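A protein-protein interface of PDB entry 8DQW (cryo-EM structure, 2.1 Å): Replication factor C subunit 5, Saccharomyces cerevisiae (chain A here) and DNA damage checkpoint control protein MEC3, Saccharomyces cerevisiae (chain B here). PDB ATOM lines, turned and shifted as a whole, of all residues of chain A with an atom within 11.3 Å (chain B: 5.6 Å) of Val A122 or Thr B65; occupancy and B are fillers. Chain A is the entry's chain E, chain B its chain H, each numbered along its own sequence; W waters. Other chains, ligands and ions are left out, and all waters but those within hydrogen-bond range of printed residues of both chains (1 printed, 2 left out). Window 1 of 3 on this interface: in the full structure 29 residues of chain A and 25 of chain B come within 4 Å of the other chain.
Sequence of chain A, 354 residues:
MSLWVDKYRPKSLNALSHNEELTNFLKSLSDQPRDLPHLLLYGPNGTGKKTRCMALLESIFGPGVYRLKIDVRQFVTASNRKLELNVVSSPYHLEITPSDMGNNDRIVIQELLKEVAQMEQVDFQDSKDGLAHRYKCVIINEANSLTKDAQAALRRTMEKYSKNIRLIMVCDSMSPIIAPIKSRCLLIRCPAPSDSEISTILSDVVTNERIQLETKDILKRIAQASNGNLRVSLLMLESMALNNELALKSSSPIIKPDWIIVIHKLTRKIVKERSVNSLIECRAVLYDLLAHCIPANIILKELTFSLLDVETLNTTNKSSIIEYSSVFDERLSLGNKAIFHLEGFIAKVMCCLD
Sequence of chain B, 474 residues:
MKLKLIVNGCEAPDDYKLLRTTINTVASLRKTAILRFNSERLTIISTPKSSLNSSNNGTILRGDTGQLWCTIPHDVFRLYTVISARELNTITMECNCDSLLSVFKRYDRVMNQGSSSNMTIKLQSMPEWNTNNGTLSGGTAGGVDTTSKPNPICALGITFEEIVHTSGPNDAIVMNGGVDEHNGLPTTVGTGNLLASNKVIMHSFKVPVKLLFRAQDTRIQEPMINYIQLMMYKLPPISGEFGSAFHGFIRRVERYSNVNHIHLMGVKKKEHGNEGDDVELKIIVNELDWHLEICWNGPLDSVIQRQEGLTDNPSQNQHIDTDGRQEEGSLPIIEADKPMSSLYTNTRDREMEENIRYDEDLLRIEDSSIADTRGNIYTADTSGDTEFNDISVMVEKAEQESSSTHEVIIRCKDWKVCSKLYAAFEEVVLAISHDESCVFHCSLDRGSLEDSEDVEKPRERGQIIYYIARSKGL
The side-chain sulfur of Met A119 sits at hydrogen-bond distance from the backbone NH of Gly B63, 3.8 Å away. The side-chain carboxylate of Glu A120 lies within salt-bridge range of the guanidinium group of Arg B470 (3.2 Å). The backbone NH (N) of Val B395 lies within hydrogen-bond range of the backbone carbonyl oxygen (O) of Leu A131 (3.4 Å).
The side-chain amino group (NZ) of Lys A136 lies close to the backbone carbonyl oxygen (O) of Met A119, 3.4 Å away. O of Gly B63 is in hydrogen-bond range of NH2 of Arg B411, 2.6 Å away. The backbone carbonyl oxygen (O) of Gln B67 lies within hydrogen-bond range of the backbone NH (N) of Tyr B467 (2.9 Å).
Among the printed residues, pairs that only touch across the chains: Val A122 with Thr B65 (3.0 Å), Phe A124 with Thr B65 (3.2 Å), Phe A124 with Tyr B467 (3.5 Å), Phe A124 with Gln B67 (3.5 Å), Phe A124 with Ala B469 (3.6 Å), Val A122 with Val B395 (3.7 Å), Leu A131 with Ala B469 (3.8 Å) and Val A122 with Arg B470 (3.99 Å).
Of the printed residues of chain B, Val A122 touches Thr B65, Val B395 and Arg B470. Thr B65 touches just these residues of chain A: Val A122 (3.0 Å) and Phe A124 (3.2 Å). Of chain A, only Met A119 comes within 4 Å of Gly B63. Gln B67 touches just one residue of chain A: Phe A124 (3.5 Å). Of chain A, only Phe A124 and Leu A131 come within 4 Å of Ala B469. Of the printed residues of chain A, Tyr B467 touches Phe A124 (3.5 Å). Printed residues of chain B within 4 Å of Leu A131: Val B395 (3.4 Å) and Ala B469 (3.8 Å). Printed residues of chain B within 4 Å of Met A119: Gly B63 (3.8 Å). Gln A121 touches none of the printed residues of chain B. Arg B411 touches none of the printed residues of chain A. The nearest printed residue of chain A that does not touch Tyr B467 is Leu A131 (7.8 Å).
Of the 23 printed residues of chain A, 5 touch a printed residue of chain B. Hydrophobic or aromatic side chains of chain A within 4 Å of the printed part of chain B: Met A119, Val A122, Phe A124 and Leu A131. Of the 13 printed residues of chain B, 7 touch a printed residue of chain A. Hydrophobic or aromatic side chains of chain B within 4 Å of the printed part of chain A: Val B395, Tyr B467 and Ala B469.
Water W1 lies within hydrogen-bond range of the side-chain amino group of Lys A136 (2.9 Å), the side-chain sulfur of Met A119 (3.0 Å) and the backbone carbonyl oxygen of Thr B59 (3.0 Å).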
ATOM      1  N   PRO A  91     -16.743 -21.829   4.263  1.00  0.00           N
ATOM      2  CA  PRO A  91     -17.217 -22.146   2.906  1.00  0.00           C
ATOM      3  C   PRO A  91     -16.831 -21.115   1.853  1.00  0.00           C
ATOM      4  O   PRO A  91     -17.002 -21.369   0.656  1.00  0.00           O
ATOM      5  CB  PRO A  91     -18.743 -22.225   3.072  1.00  0.00           C
ATOM      6  CG  PRO A  91     -19.046 -21.582   4.385  1.00  0.00           C
ATOM      7  CD  PRO A  91     -17.843 -21.764   5.240  1.00  0.00           C
ATOM      8  N   VAL A 116      -4.293 -24.157  -4.644  1.00  0.00           N
ATOM      9  CA  VAL A 116      -5.533 -23.428  -4.399  1.00  0.00           C
ATOM     10  C   VAL A 116      -5.739 -22.376  -5.478  1.00  0.00           C
ATOM     11  O   VAL A 116      -6.856 -22.180  -5.972  1.00  0.00           O
ATOM     12  CB  VAL A 116      -5.516 -22.802  -2.992  1.00  0.00           C
ATOM     13  CG1 VAL A 116      -6.683 -21.837  -2.823  1.00  0.00           C
ATOM     14  CG2 VAL A 116      -5.555 -23.887  -1.926  1.00  0.00           C
ATOM     15  N   ALA A 117      -4.663 -21.687  -5.866  1.00  0.00           N
ATOM     16  CA  ALA A 117      -4.776 -20.682  -6.914  1.00  0.00           C
ATOM     17  C   ALA A 117      -5.117 -21.311  -8.258  1.00  0.00           C
ATOM     18  O   ALA A 117      -5.836 -20.704  -9.058  1.00  0.00           O
ATOM     19  CB  ALA A 117      -3.477 -19.883  -7.016  1.00  0.00           C
ATOM     20  N   GLN A 118      -4.613 -22.519  -8.523  1.00  0.00           N
ATOM     21  CA  GLN A 118      -4.812 -23.132  -9.831  1.00  0.00           C
ATOM     22  C   GLN A 118      -6.214 -23.704  -9.995  1.00  0.00           C
ATOM     23  O   GLN A 118      -6.769 -23.660 -11.099  1.00  0.00           O
ATOM     24  CB  GLN A 118      -3.765 -24.223 -10.056  1.00  0.00           C
ATOM     25  CG  GLN A 118      -2.435 -23.688 -10.558  1.00  0.00           C
ATOM     26  CD  GLN A 118      -1.350 -24.744 -10.588  1.00  0.00           C
ATOM     27  OE1 GLN A 118      -1.487 -25.810  -9.990  1.00  0.00           O
ATOM     28  NE2 GLN A 118      -0.259 -24.449 -11.285  1.00  0.00           N
ATOM     29  N   MET A 119      -6.799 -24.237  -8.926  1.00  0.00           N
ATOM     30  CA  MET A 119      -8.132 -24.828  -8.993  1.00  0.00           C
ATOM     31  C   MET A 119      -9.158 -23.703  -9.045  1.00  0.00           C
ATOM     32  O   MET A 119      -9.363 -22.991  -8.057  1.00  0.00           O
ATOM     33  CB  MET A 119      -8.365 -25.744  -7.793  1.00  0.00           C
ATOM     34  CG  MET A 119      -9.834 -26.043  -7.485  1.00  0.00           C
ATOM     35  SD  MET A 119     -10.069 -26.984  -5.962  1.00  0.00           S
ATOM     36  CE  MET A 119      -8.845 -28.277  -6.142  1.00  0.00           C
ATOM     37  N   GLU A 120      -9.806 -23.540 -10.196  1.00  0.00           N
ATOM     38  CA  GLU A 120     -10.811 -22.499 -10.360  1.00  0.00           C
ATOM     39  C   GLU A 120     -12.132 -22.962  -9.757  1.00  0.00           C
ATOM     40  O   GLU A 120     -12.594 -24.076 -10.029  1.00  0.00           O
ATOM     41  CB  GLU A 120     -10.970 -22.146 -11.840  1.00  0.00           C
ATOM     42  CG  GLU A 120     -12.393 -21.846 -12.279  1.00  0.00           C
ATOM     43  CD  GLU A 120     -12.478 -21.434 -13.735  1.00  0.00           C
ATOM     44  OE1 GLU A 120     -11.807 -22.068 -14.576  1.00  0.00           O
ATOM     45  OE2 GLU A 120     -13.221 -20.478 -14.039  1.00  0.00           O
ATOM     46  N   GLN A 121     -12.738 -22.107  -8.937  1.00  0.00           N
ATOM     47  CA  GLN A 121     -13.934 -22.462  -8.181  1.00  0.00           C
ATOM     48  C   GLN A 121     -15.167 -22.121  -9.011  1.00  0.00           C
ATOM     49  O   GLN A 121     -15.445 -20.947  -9.273  1.00  0.00           O
ATOM     50  CB  GLN A 121     -13.944 -21.734  -6.837  1.00  0.00           C
ATOM     51  CG  GLN A 121     -15.208 -21.930  -6.014  1.00  0.00           C
ATOM     52  CD  GLN A 121     -15.185 -21.136  -4.722  1.00  0.00           C
ATOM     53  OE1 GLN A 121     -14.931 -19.932  -4.722  1.00  0.00           O
ATOM     54  NE2 GLN A 121     -15.444 -21.813  -3.608  1.00  0.00           N
ATOM     55  N   VAL A 122     -15.907 -23.153  -9.421  1.00  0.00           N
ATOM     56  CA  VAL A 122     -17.132 -22.996 -10.193  1.00  0.00           C
ATOM     57  C   VAL A 122     -18.240 -23.774  -9.497  1.00  0.00           C
ATOM     58  O   VAL A 122     -17.990 -24.699  -8.722  1.00  0.00           O
ATOM     59  CB  VAL A 122     -16.974 -23.475 -11.652  1.00  0.00           C
ATOM     60  CG1 VAL A 122     -15.881 -22.689 -12.353  1.00  0.00           C
ATOM     61  CG2 VAL A 122     -16.680 -24.968 -11.699  1.00  0.00           C
ATOM     62  N   ASP A 123     -19.480 -23.381  -9.779  1.00  0.00           N
ATOM     63  CA  ASP A 123     -20.627 -24.034  -9.164  1.00  0.00           C
ATOM     64  C   ASP A 123     -21.831 -23.943 -10.091  1.00  0.00           C
ATOM     65  O   ASP A 123     -21.977 -22.984 -10.852  1.00  0.00           O
ATOM     66  CB  ASP A 123     -20.953 -23.407  -7.801  1.00  0.00           C
ATOM     67  CG  ASP A 123     -22.390 -23.636  -7.379  1.00  0.00           C
ATOM     68  OD1 ASP A 123     -23.036 -22.672  -6.917  1.00  0.00           O
ATOM     69  OD2 ASP A 123     -22.874 -24.782  -7.503  1.00  0.00           O
ATOM     70  N   PHE A 124     -22.698 -24.951 -10.017  1.00  0.00           N
ATOM     71  CA  PHE A 124     -23.940 -24.919 -10.778  1.00  0.00           C
ATOM     72  C   PHE A 124     -24.806 -23.750 -10.322  1.00  0.00           C
ATOM     73  O   PHE A 124     -24.942 -23.484  -9.126  1.00  0.00           O
ATOM     74  CB  PHE A 124     -24.703 -26.234 -10.607  1.00  0.00           C
ATOM     75  CG  PHE A 124     -24.024 -27.419 -11.237  1.00  0.00           C
ATOM     76  CD1 PHE A 124     -24.021 -27.584 -12.611  1.00  0.00           C
ATOM     77  CD2 PHE A 124     -23.395 -28.370 -10.452  1.00  0.00           C
ATOM     78  CE1 PHE A 124     -23.400 -28.673 -13.192  1.00  0.00           C
ATOM     79  CE2 PHE A 124     -22.773 -29.462 -11.028  1.00  0.00           C
ATOM     80  CZ  PHE A 124     -22.776 -29.613 -12.399  1.00  0.00           C
ATOM     81  N   GLN A 125     -25.396 -23.049 -11.289  1.00  0.00           N
ATOM     82  CA  GLN A 125     -26.237 -21.897 -10.987  1.00  0.00           C
ATOM     83  C   GLN A 125     -27.633 -22.361 -10.593  1.00  0.00           C
ATOM     84  O   GLN A 125     -28.243 -23.185 -11.281  1.00  0.00           O
ATOM     85  CB  GLN A 125     -26.305 -20.957 -12.189  1.00  0.00           C
ATOM     86  CG  GLN A 125     -25.150 -19.971 -12.256  1.00  0.00           C
ATOM     87  CD  GLN A 125     -25.340 -18.916 -13.326  1.00  0.00           C
ATOM     88  OE1 GLN A 125     -25.480 -19.233 -14.507  1.00  0.00           O
ATOM     89  NE2 GLN A 125     -25.348 -17.653 -12.918  1.00  0.00           N
ATOM     90  N   ASP A 126     -28.137 -21.825  -9.478  1.00  0.00           N
ATOM     91  CA  ASP A 126     -29.427 -22.271  -8.958  1.00  0.00           C
ATOM     92  C   ASP A 126     -30.565 -21.940  -9.916  1.00  0.00           C
ATOM     93  O   ASP A 126     -31.458 -22.765 -10.138  1.00  0.00           O
ATOM     94  CB  ASP A 126     -29.681 -21.637  -7.589  1.00  0.00           C
ATOM     95  CG  ASP A 126     -30.543 -22.508  -6.691  1.00  0.00           C
ATOM     96  OD1 ASP A 126     -30.667 -23.720  -6.963  1.00  0.00           O
ATOM     97  OD2 ASP A 126     -31.098 -21.975  -5.706  1.00  0.00           O
ATOM     98  N   ASP A 129     -28.543 -19.969 -16.261  1.00  0.00           N
ATOM     99  CA  ASP A 129     -28.005 -21.008 -17.126  1.00  0.00           C
ATOM    100  C   ASP A 129     -26.483 -20.956 -17.130  1.00  0.00           C
ATOM    101  O   ASP A 129     -25.887 -19.886 -17.284  1.00  0.00           O
ATOM    102  CB  ASP A 129     -28.535 -20.856 -18.553  1.00  0.00           C
ATOM    103  CG  ASP A 129     -30.049 -20.864 -18.615  1.00  0.00           C
ATOM    104  OD1 ASP A 129     -30.688 -21.055 -17.559  1.00  0.00           O
ATOM    105  OD2 ASP A 129     -30.602 -20.682 -19.721  1.00  0.00           O
ATOM    106  N   GLY A 130     -25.862 -22.120 -16.957  1.00  0.00           N
ATOM    107  CA  GLY A 130     -24.418 -22.219 -16.952  1.00  0.00           C
ATOM    108  C   GLY A 130     -23.834 -22.121 -15.559  1.00  0.00           C
ATOM    109  O   GLY A 130     -24.502 -21.787 -14.577  1.00  0.00           O
ATOM    110  N   LEU A 131     -22.544 -22.431 -15.478  1.00  0.00           N
ATOM    111  CA  LEU A 131     -21.820 -22.388 -14.217  1.00  0.00           C
ATOM    112  C   LEU A 131     -21.496 -20.952 -13.831  1.00  0.00           C
ATOM    113  O   LEU A 131     -21.375 -20.067 -14.682  1.00  0.00           O
ATOM    114  CB  LEU A 131     -20.527 -23.200 -14.303  1.00  0.00           C
ATOM    115  CG  LEU A 131     -20.643 -24.645 -14.786  1.00  0.00           C
ATOM    116  CD1 LEU A 131     -19.319 -25.108 -15.371  1.00  0.00           C
ATOM    117  CD2 LEU A 131     -21.079 -25.556 -13.650  1.00  0.00           C
ATOM    118  N   ALA A 132     -21.355 -20.731 -12.527  1.00  0.00           N
ATOM    119  CA  ALA A 132     -20.958 -19.449 -11.971  1.00  0.00           C
ATOM    120  C   ALA A 132     -19.583 -19.583 -11.333  1.00  0.00           C
ATOM    121  O   ALA A 132     -19.273 -20.606 -10.712  1.00  0.00           O
ATOM    122  CB  ALA A 132     -21.971 -18.958 -10.933  1.00  0.00           C
ATOM    123  N   HIS A 133     -18.767 -18.547 -11.495  1.00  0.00           N
ATOM    124  CA  HIS A 133     -17.402 -18.517 -10.991  1.00  0.00           C
ATOM    125  C   HIS A 133     -17.293 -17.516  -9.848  1.00  0.00           C
ATOM    126  O   HIS A 133     -17.951 -16.473  -9.859  1.00  0.00           O
ATOM    127  CB  HIS A 133     -16.420 -18.147 -12.106  1.00  0.00           C
ATOM    128  CG  HIS A 133     -15.017 -17.934 -11.629  1.00  0.00           C
ATOM    129  ND1 HIS A 133     -14.427 -16.690 -11.586  1.00  0.00           N
ATOM    130  CD2 HIS A 133     -14.091 -18.807 -11.169  1.00  0.00           C
ATOM    131  CE1 HIS A 133     -13.193 -16.806 -11.126  1.00  0.00           C
ATOM    132  NE2 HIS A 133     -12.966 -18.080 -10.865  1.00  0.00           N
ATOM    133  N   ARG A 134     -16.459 -17.845  -8.864  1.00  0.00           N
ATOM    134  CA  ARG A 134     -16.239 -16.993  -7.702  1.00  0.00           C
ATOM    135  C   ARG A 134     -14.793 -17.139  -7.256  1.00  0.00           C
ATOM    136  O   ARG A 134     -14.301 -18.261  -7.112  1.00  0.00           O
ATOM    137  CB  ARG A 134     -17.185 -17.370  -6.557  1.00  0.00           C
ATOM    138  CG  ARG A 134     -18.513 -16.628  -6.573  1.00  0.00           C
ATOM    139  CD  ARG A 134     -19.444 -17.094  -5.457  1.00  0.00           C
ATOM    140  NE  ARG A 134     -19.040 -18.373  -4.883  1.00  0.00           N
ATOM    141  CZ  ARG A 134     -19.570 -19.549  -5.194  1.00  0.00           C
ATOM    142  NH1 ARG A 134     -20.539 -19.661  -6.090  1.00  0.00           N
ATOM    143  NH2 ARG A 134     -19.112 -20.645  -4.596  1.00  0.00           N
ATOM    144  N   TYR A 135     -14.117 -16.015  -7.035  1.00  0.00           N
ATOM    145  CA  TYR A 135     -12.737 -16.077  -6.576  1.00  0.00           C
ATOM    146  C   TYR A 135     -12.684 -16.502  -5.113  1.00  0.00           C
ATOM    147  O   TYR A 135     -13.595 -16.230  -4.327  1.00  0.00           O
ATOM    148  CB  TYR A 135     -12.029 -14.733  -6.780  1.00  0.00           C
ATOM    149  CG  TYR A 135     -12.548 -13.563  -5.959  1.00  0.00           C
ATOM    150  CD1 TYR A 135     -12.388 -13.522  -4.578  1.00  0.00           C
ATOM    151  CD2 TYR A 135     -13.168 -12.484  -6.576  1.00  0.00           C
ATOM    152  CE1 TYR A 135     -12.851 -12.452  -3.836  1.00  0.00           C
ATOM    153  CE2 TYR A 135     -13.632 -11.409  -5.842  1.00  0.00           C
ATOM    154  CZ  TYR A 135     -13.470 -11.397  -4.472  1.00  0.00           C
ATOM    155  OH  TYR A 135     -13.930 -10.329  -3.738  1.00  0.00           O
ATOM    156  N   LYS A 136     -11.603 -17.190  -4.756  1.00  0.00           N
ATOM    157  CA  LYS A 136     -11.383 -17.634  -3.389  1.00  0.00           C
ATOM    158  C   LYS A 136     -10.609 -16.570  -2.621  1.00  0.00           C
ATOM    159  O   LYS A 136      -9.761 -15.873  -3.185  1.00  0.00           O
ATOM    160  CB  LYS A 136     -10.612 -18.955  -3.362  1.00  0.00           C
ATOM    161  CG  LYS A 136     -11.096 -19.999  -4.358  1.00  0.00           C
ATOM    162  CD  LYS A 136     -10.077 -21.120  -4.515  1.00  0.00           C
ATOM    163  CE  LYS A 136     -10.701 -22.377  -5.094  1.00  0.00           C
ATOM    164  NZ  LYS A 136      -9.894 -23.589  -4.796  1.00  0.00           N
ATOM    165  N   LYS A 163      -7.700 -14.133 -11.176  1.00  0.00           N
ATOM    166  CA  LYS A 163      -9.122 -14.402 -11.358  1.00  0.00           C
ATOM    167  C   LYS A 163      -9.661 -15.342 -10.287  1.00  0.00           C
ATOM    168  O   LYS A 163     -10.823 -15.219  -9.885  1.00  0.00           O
ATOM    169  CB  LYS A 163      -9.369 -14.997 -12.744  1.00  0.00           C
ATOM    170  CG  LYS A 163      -9.839 -13.995 -13.785  1.00  0.00           C
ATOM    171  CD  LYS A 163      -9.773 -14.584 -15.191  1.00  0.00           C
ATOM    172  CE  LYS A 163      -9.355 -13.542 -16.213  1.00  0.00           C
ATOM    173  NZ  LYS A 163     -10.275 -12.374 -16.224  1.00  0.00           N
ATOM    174  N   ASN A 164      -8.841 -16.282  -9.817  1.00  0.00           N
ATOM    175  CA  ASN A 164      -9.301 -17.322  -8.908  1.00  0.00           C
ATOM    176  C   ASN A 164      -9.064 -17.009  -7.437  1.00  0.00           C
ATOM    177  O   ASN A 164      -9.779 -17.551  -6.588  1.00  0.00           O
ATOM    178  CB  ASN A 164      -8.614 -18.655  -9.237  1.00  0.00           C
ATOM    179  CG  ASN A 164      -8.787 -19.060 -10.689  1.00  0.00           C
ATOM    180  OD1 ASN A 164      -9.561 -18.453 -11.429  1.00  0.00           O
ATOM    181  ND2 ASN A 164      -8.066 -20.095 -11.103  1.00  0.00           N
ATOM    182  N   ILE A 165      -8.090 -16.160  -7.110  1.00  0.00           N
ATOM    183  CA  ILE A 165      -7.673 -15.955  -5.728  1.00  0.00           C
ATOM    184  C   ILE A 165      -7.468 -14.471  -5.457  1.00  0.00           C
ATOM    185  O   ILE A 165      -7.086 -13.701  -6.344  1.00  0.00           O
ATOM    186  CB  ILE A 165      -6.384 -16.745  -5.409  1.00  0.00           C
ATOM    187  CG1 ILE A 165      -6.216 -16.916  -3.897  1.00  0.00           C
ATOM    188  CG2 ILE A 165      -5.168 -16.050  -6.008  1.00  0.00           C
ATOM    189  CD1 ILE A 165      -5.230 -17.997  -3.519  1.00  0.00           C
ATOM    190  N   ARG B  30     -21.065 -38.527  -1.081  1.00  0.00           N
ATOM    191  CA  ARG B  30     -21.023 -37.593   0.035  1.00  0.00           C
ATOM    192  C   ARG B  30     -21.489 -38.299   1.301  1.00  0.00           C
ATOM    193  O   ARG B  30     -22.061 -39.392   1.260  1.00  0.00           O
ATOM    194  CB  ARG B  30     -21.881 -36.352  -0.242  1.00  0.00           C
ATOM    195  CG  ARG B  30     -21.069 -35.111  -0.582  1.00  0.00           C
ATOM    196  CD  ARG B  30     -21.949 -33.992  -1.113  1.00  0.00           C
ATOM    197  NE  ARG B  30     -22.569 -34.336  -2.388  1.00  0.00           N
ATOM    198  CZ  ARG B  30     -22.033 -34.097  -3.577  1.00  0.00           C
ATOM    199  NH1 ARG B  30     -20.851 -33.512  -3.701  1.00  0.00           N
ATOM    200  NH2 ARG B  30     -22.698 -34.453  -4.672  1.00  0.00           N
ATOM    201  N   PRO B  48     -23.621 -30.776  -2.645  1.00  0.00           N
ATOM    202  CA  PRO B  48     -22.824 -30.076  -1.628  1.00  0.00           C
ATOM    203  C   PRO B  48     -23.537 -28.898  -0.988  1.00  0.00           C
ATOM    204  O   PRO B  48     -23.015 -28.336  -0.015  1.00  0.00           O
ATOM    205  CB  PRO B  48     -21.595 -29.607  -2.417  1.00  0.00           C
ATOM    206  CG  PRO B  48     -22.093 -29.430  -3.804  1.00  0.00           C
ATOM    207  CD  PRO B  48     -23.163 -30.468  -4.012  1.00  0.00           C
ATOM    208  N   THR B  59     -16.569 -27.608  -1.650  1.00  0.00           N
ATOM    209  CA  THR B  59     -16.469 -26.881  -2.911  1.00  0.00           C
ATOM    210  C   THR B  59     -15.191 -26.051  -2.971  1.00  0.00           C
ATOM    211  O   THR B  59     -14.487 -26.048  -3.987  1.00  0.00           O
ATOM    212  CB  THR B  59     -17.696 -25.988  -3.097  1.00  0.00           C
ATOM    213  OG1 THR B  59     -18.884 -26.786  -3.046  1.00  0.00           O
ATOM    214  CG2 THR B  59     -17.634 -25.257  -4.431  1.00  0.00           C
ATOM    215  N   GLY B  63     -13.123 -28.803  -4.668  1.00  0.00           N
ATOM    216  CA  GLY B  63     -13.956 -28.686  -5.849  1.00  0.00           C
ATOM    217  C   GLY B  63     -14.961 -29.810  -6.003  1.00  0.00           C
ATOM    218  O   GLY B  63     -15.096 -30.380  -7.090  1.00  0.00           O
ATOM    219  N   ASP B  64     -15.670 -30.143  -4.925  1.00  0.00           N
ATOM    220  CA  ASP B  64     -16.714 -31.169  -4.963  1.00  0.00           C
ATOM    221  C   ASP B  64     -18.011 -30.498  -5.393  1.00  0.00           C
ATOM    222  O   ASP B  64     -18.826 -30.080  -4.568  1.00  0.00           O
ATOM    223  CB  ASP B  64     -16.856 -31.852  -3.609  1.00  0.00           C
ATOM    224  CG  ASP B  64     -15.520 -32.159  -2.967  1.00  0.00           C
ATOM    225  OD1 ASP B  64     -14.816 -31.204  -2.579  1.00  0.00           O
ATOM    226  OD2 ASP B  64     -15.174 -33.353  -2.850  1.00  0.00           O
ATOM    227  N   THR B  65     -18.208 -30.398  -6.707  1.00  0.00           N
ATOM    228  CA  THR B  65     -19.348 -29.695  -7.274  1.00  0.00           C
ATOM    229  C   THR B  65     -20.380 -30.616  -7.909  1.00  0.00           C
ATOM    230  O   THR B  65     -21.498 -30.165  -8.183  1.00  0.00           O
ATOM    231  CB  THR B  65     -18.875 -28.684  -8.329  1.00  0.00           C
ATOM    232  OG1 THR B  65     -17.855 -29.279  -9.142  1.00  0.00           O
ATOM    233  CG2 THR B  65     -18.324 -27.437  -7.662  1.00  0.00           C
ATOM    234  N   GLY B  66     -20.045 -31.880  -8.151  1.00  0.00           N
ATOM    235  CA  GLY B  66     -20.976 -32.771  -8.812  1.00  0.00           C
ATOM    236  C   GLY B  66     -22.216 -33.025  -7.975  1.00  0.00           C
ATOM    237  O   GLY B  66     -22.174 -33.053  -6.746  1.00  0.00           O
ATOM    238  N   GLN B  67     -23.340 -33.216  -8.663  1.00  0.00           N
ATOM    239  CA  GLN B  67     -24.628 -33.420  -8.010  1.00  0.00           C
ATOM    240  C   GLN B  67     -25.272 -34.690  -8.542  1.00  0.00           C
ATOM    241  O   GLN B  67     -25.340 -34.892  -9.758  1.00  0.00           O
ATOM    242  CB  GLN B  67     -25.558 -32.223  -8.235  1.00  0.00           C
ATOM    243  CG  GLN B  67     -25.033 -30.915  -7.665  1.00  0.00           C
ATOM    244  CD  GLN B  67     -26.096 -29.836  -7.604  1.00  0.00           C
ATOM    245  OE1 GLN B  67     -27.277 -30.121  -7.411  1.00  0.00           O
ATOM    246  NE2 GLN B  67     -25.679 -28.586  -7.769  1.00  0.00           N
ATOM    247  N   VAL B 395     -18.789 -18.372 -16.069  1.00  0.00           N
ATOM    248  CA  VAL B 395     -17.514 -18.966 -16.450  1.00  0.00           C
ATOM    249  C   VAL B 395     -17.201 -18.624 -17.902  1.00  0.00           C
ATOM    250  O   VAL B 395     -18.100 -18.432 -18.731  1.00  0.00           O
ATOM    251  CB  VAL B 395     -17.536 -20.491 -16.237  1.00  0.00           C
ATOM    252  CG1 VAL B 395     -17.862 -20.826 -14.791  1.00  0.00           C
ATOM    253  CG2 VAL B 395     -18.531 -21.151 -17.185  1.00  0.00           C
ATOM    254  N   ARG B 411     -12.715 -34.455 -13.825  1.00  0.00           N
ATOM    255  CA  ARG B 411     -11.872 -35.196 -12.901  1.00  0.00           C
ATOM    256  C   ARG B 411     -12.028 -36.699 -13.114  1.00  0.00           C
ATOM    257  O   ARG B 411     -13.052 -37.185 -13.603  1.00  0.00           O
ATOM    258  CB  ARG B 411     -12.216 -34.839 -11.454  1.00  0.00           C
ATOM    259  CG  ARG B 411     -11.437 -33.659 -10.901  1.00  0.00           C
ATOM    260  CD  ARG B 411     -11.959 -33.241  -9.535  1.00  0.00           C
ATOM    261  NE  ARG B 411     -13.255 -32.576  -9.626  1.00  0.00           N
ATOM    262  CZ  ARG B 411     -13.444 -31.263  -9.575  1.00  0.00           C
ATOM    263  NH1 ARG B 411     -12.432 -30.420  -9.439  1.00  0.00           N
ATOM    264  NH2 ARG B 411     -14.680 -30.783  -9.668  1.00  0.00           N
ATOM    265  N   TYR B 467     -24.594 -34.799 -12.541  1.00  0.00           N
ATOM    266  CA  TYR B 467     -24.037 -33.601 -13.152  1.00  0.00           C
ATOM    267  C   TYR B 467     -22.617 -33.404 -12.645  1.00  0.00           C
ATOM    268  O   TYR B 467     -22.374 -33.447 -11.433  1.00  0.00           O
ATOM    269  CB  TYR B 467     -24.881 -32.369 -12.821  1.00  0.00           C
ATOM    270  CG  TYR B 467     -26.357 -32.519 -13.107  1.00  0.00           C
ATOM    271  CD1 TYR B 467     -27.204 -33.134 -12.194  1.00  0.00           C
ATOM    272  CD2 TYR B 467     -26.907 -32.034 -14.285  1.00  0.00           C
ATOM    273  CE1 TYR B 467     -28.555 -33.269 -12.452  1.00  0.00           C
ATOM    274  CE2 TYR B 467     -28.254 -32.162 -14.551  1.00  0.00           C
ATOM    275  CZ  TYR B 467     -29.075 -32.778 -13.631  1.00  0.00           C
ATOM    276  OH  TYR B 467     -30.418 -32.907 -13.898  1.00  0.00           O
ATOM    277  N   ALA B 469     -19.394 -30.730 -13.078  1.00  0.00           N
ATOM    278  CA  ALA B 469     -18.854 -29.487 -13.596  1.00  0.00           C
ATOM    279  C   ALA B 469     -17.434 -29.707 -14.108  1.00  0.00           C
ATOM    280  O   ALA B 469     -16.730 -30.630 -13.693  1.00  0.00           O
ATOM    281  CB  ALA B 469     -18.864 -28.401 -12.519  1.00  0.00           C
ATOM    282  N   ARG B 470     -17.019 -28.844 -15.031  1.00  0.00           N
ATOM    283  CA  ARG B 470     -15.675 -28.939 -15.580  1.00  0.00           C
ATOM    284  C   ARG B 470     -14.636 -28.767 -14.479  1.00  0.00           C
ATOM    285  O   ARG B 470     -14.805 -27.958 -13.561  1.00  0.00           O
ATOM    286  CB  ARG B 470     -15.472 -27.879 -16.663  1.00  0.00           C
ATOM    287  CG  ARG B 470     -15.045 -26.525 -16.122  1.00  0.00           C
ATOM    288  CD  ARG B 470     -15.235 -25.426 -17.148  1.00  0.00           C
ATOM    289  NE  ARG B 470     -14.572 -24.192 -16.747  1.00  0.00           N
ATOM    290  CZ  ARG B 470     -14.500 -23.101 -17.496  1.00  0.00           C
ATOM    291  NH1 ARG B 470     -15.039 -23.054 -18.704  1.00  0.00           N
ATOM    292  NH2 ARG B 470     -13.872 -22.029 -17.023  1.00  0.00           N
HETATM  293  O   HOH W   1     -12.237 -24.964  -5.725  1.00  0.00           O
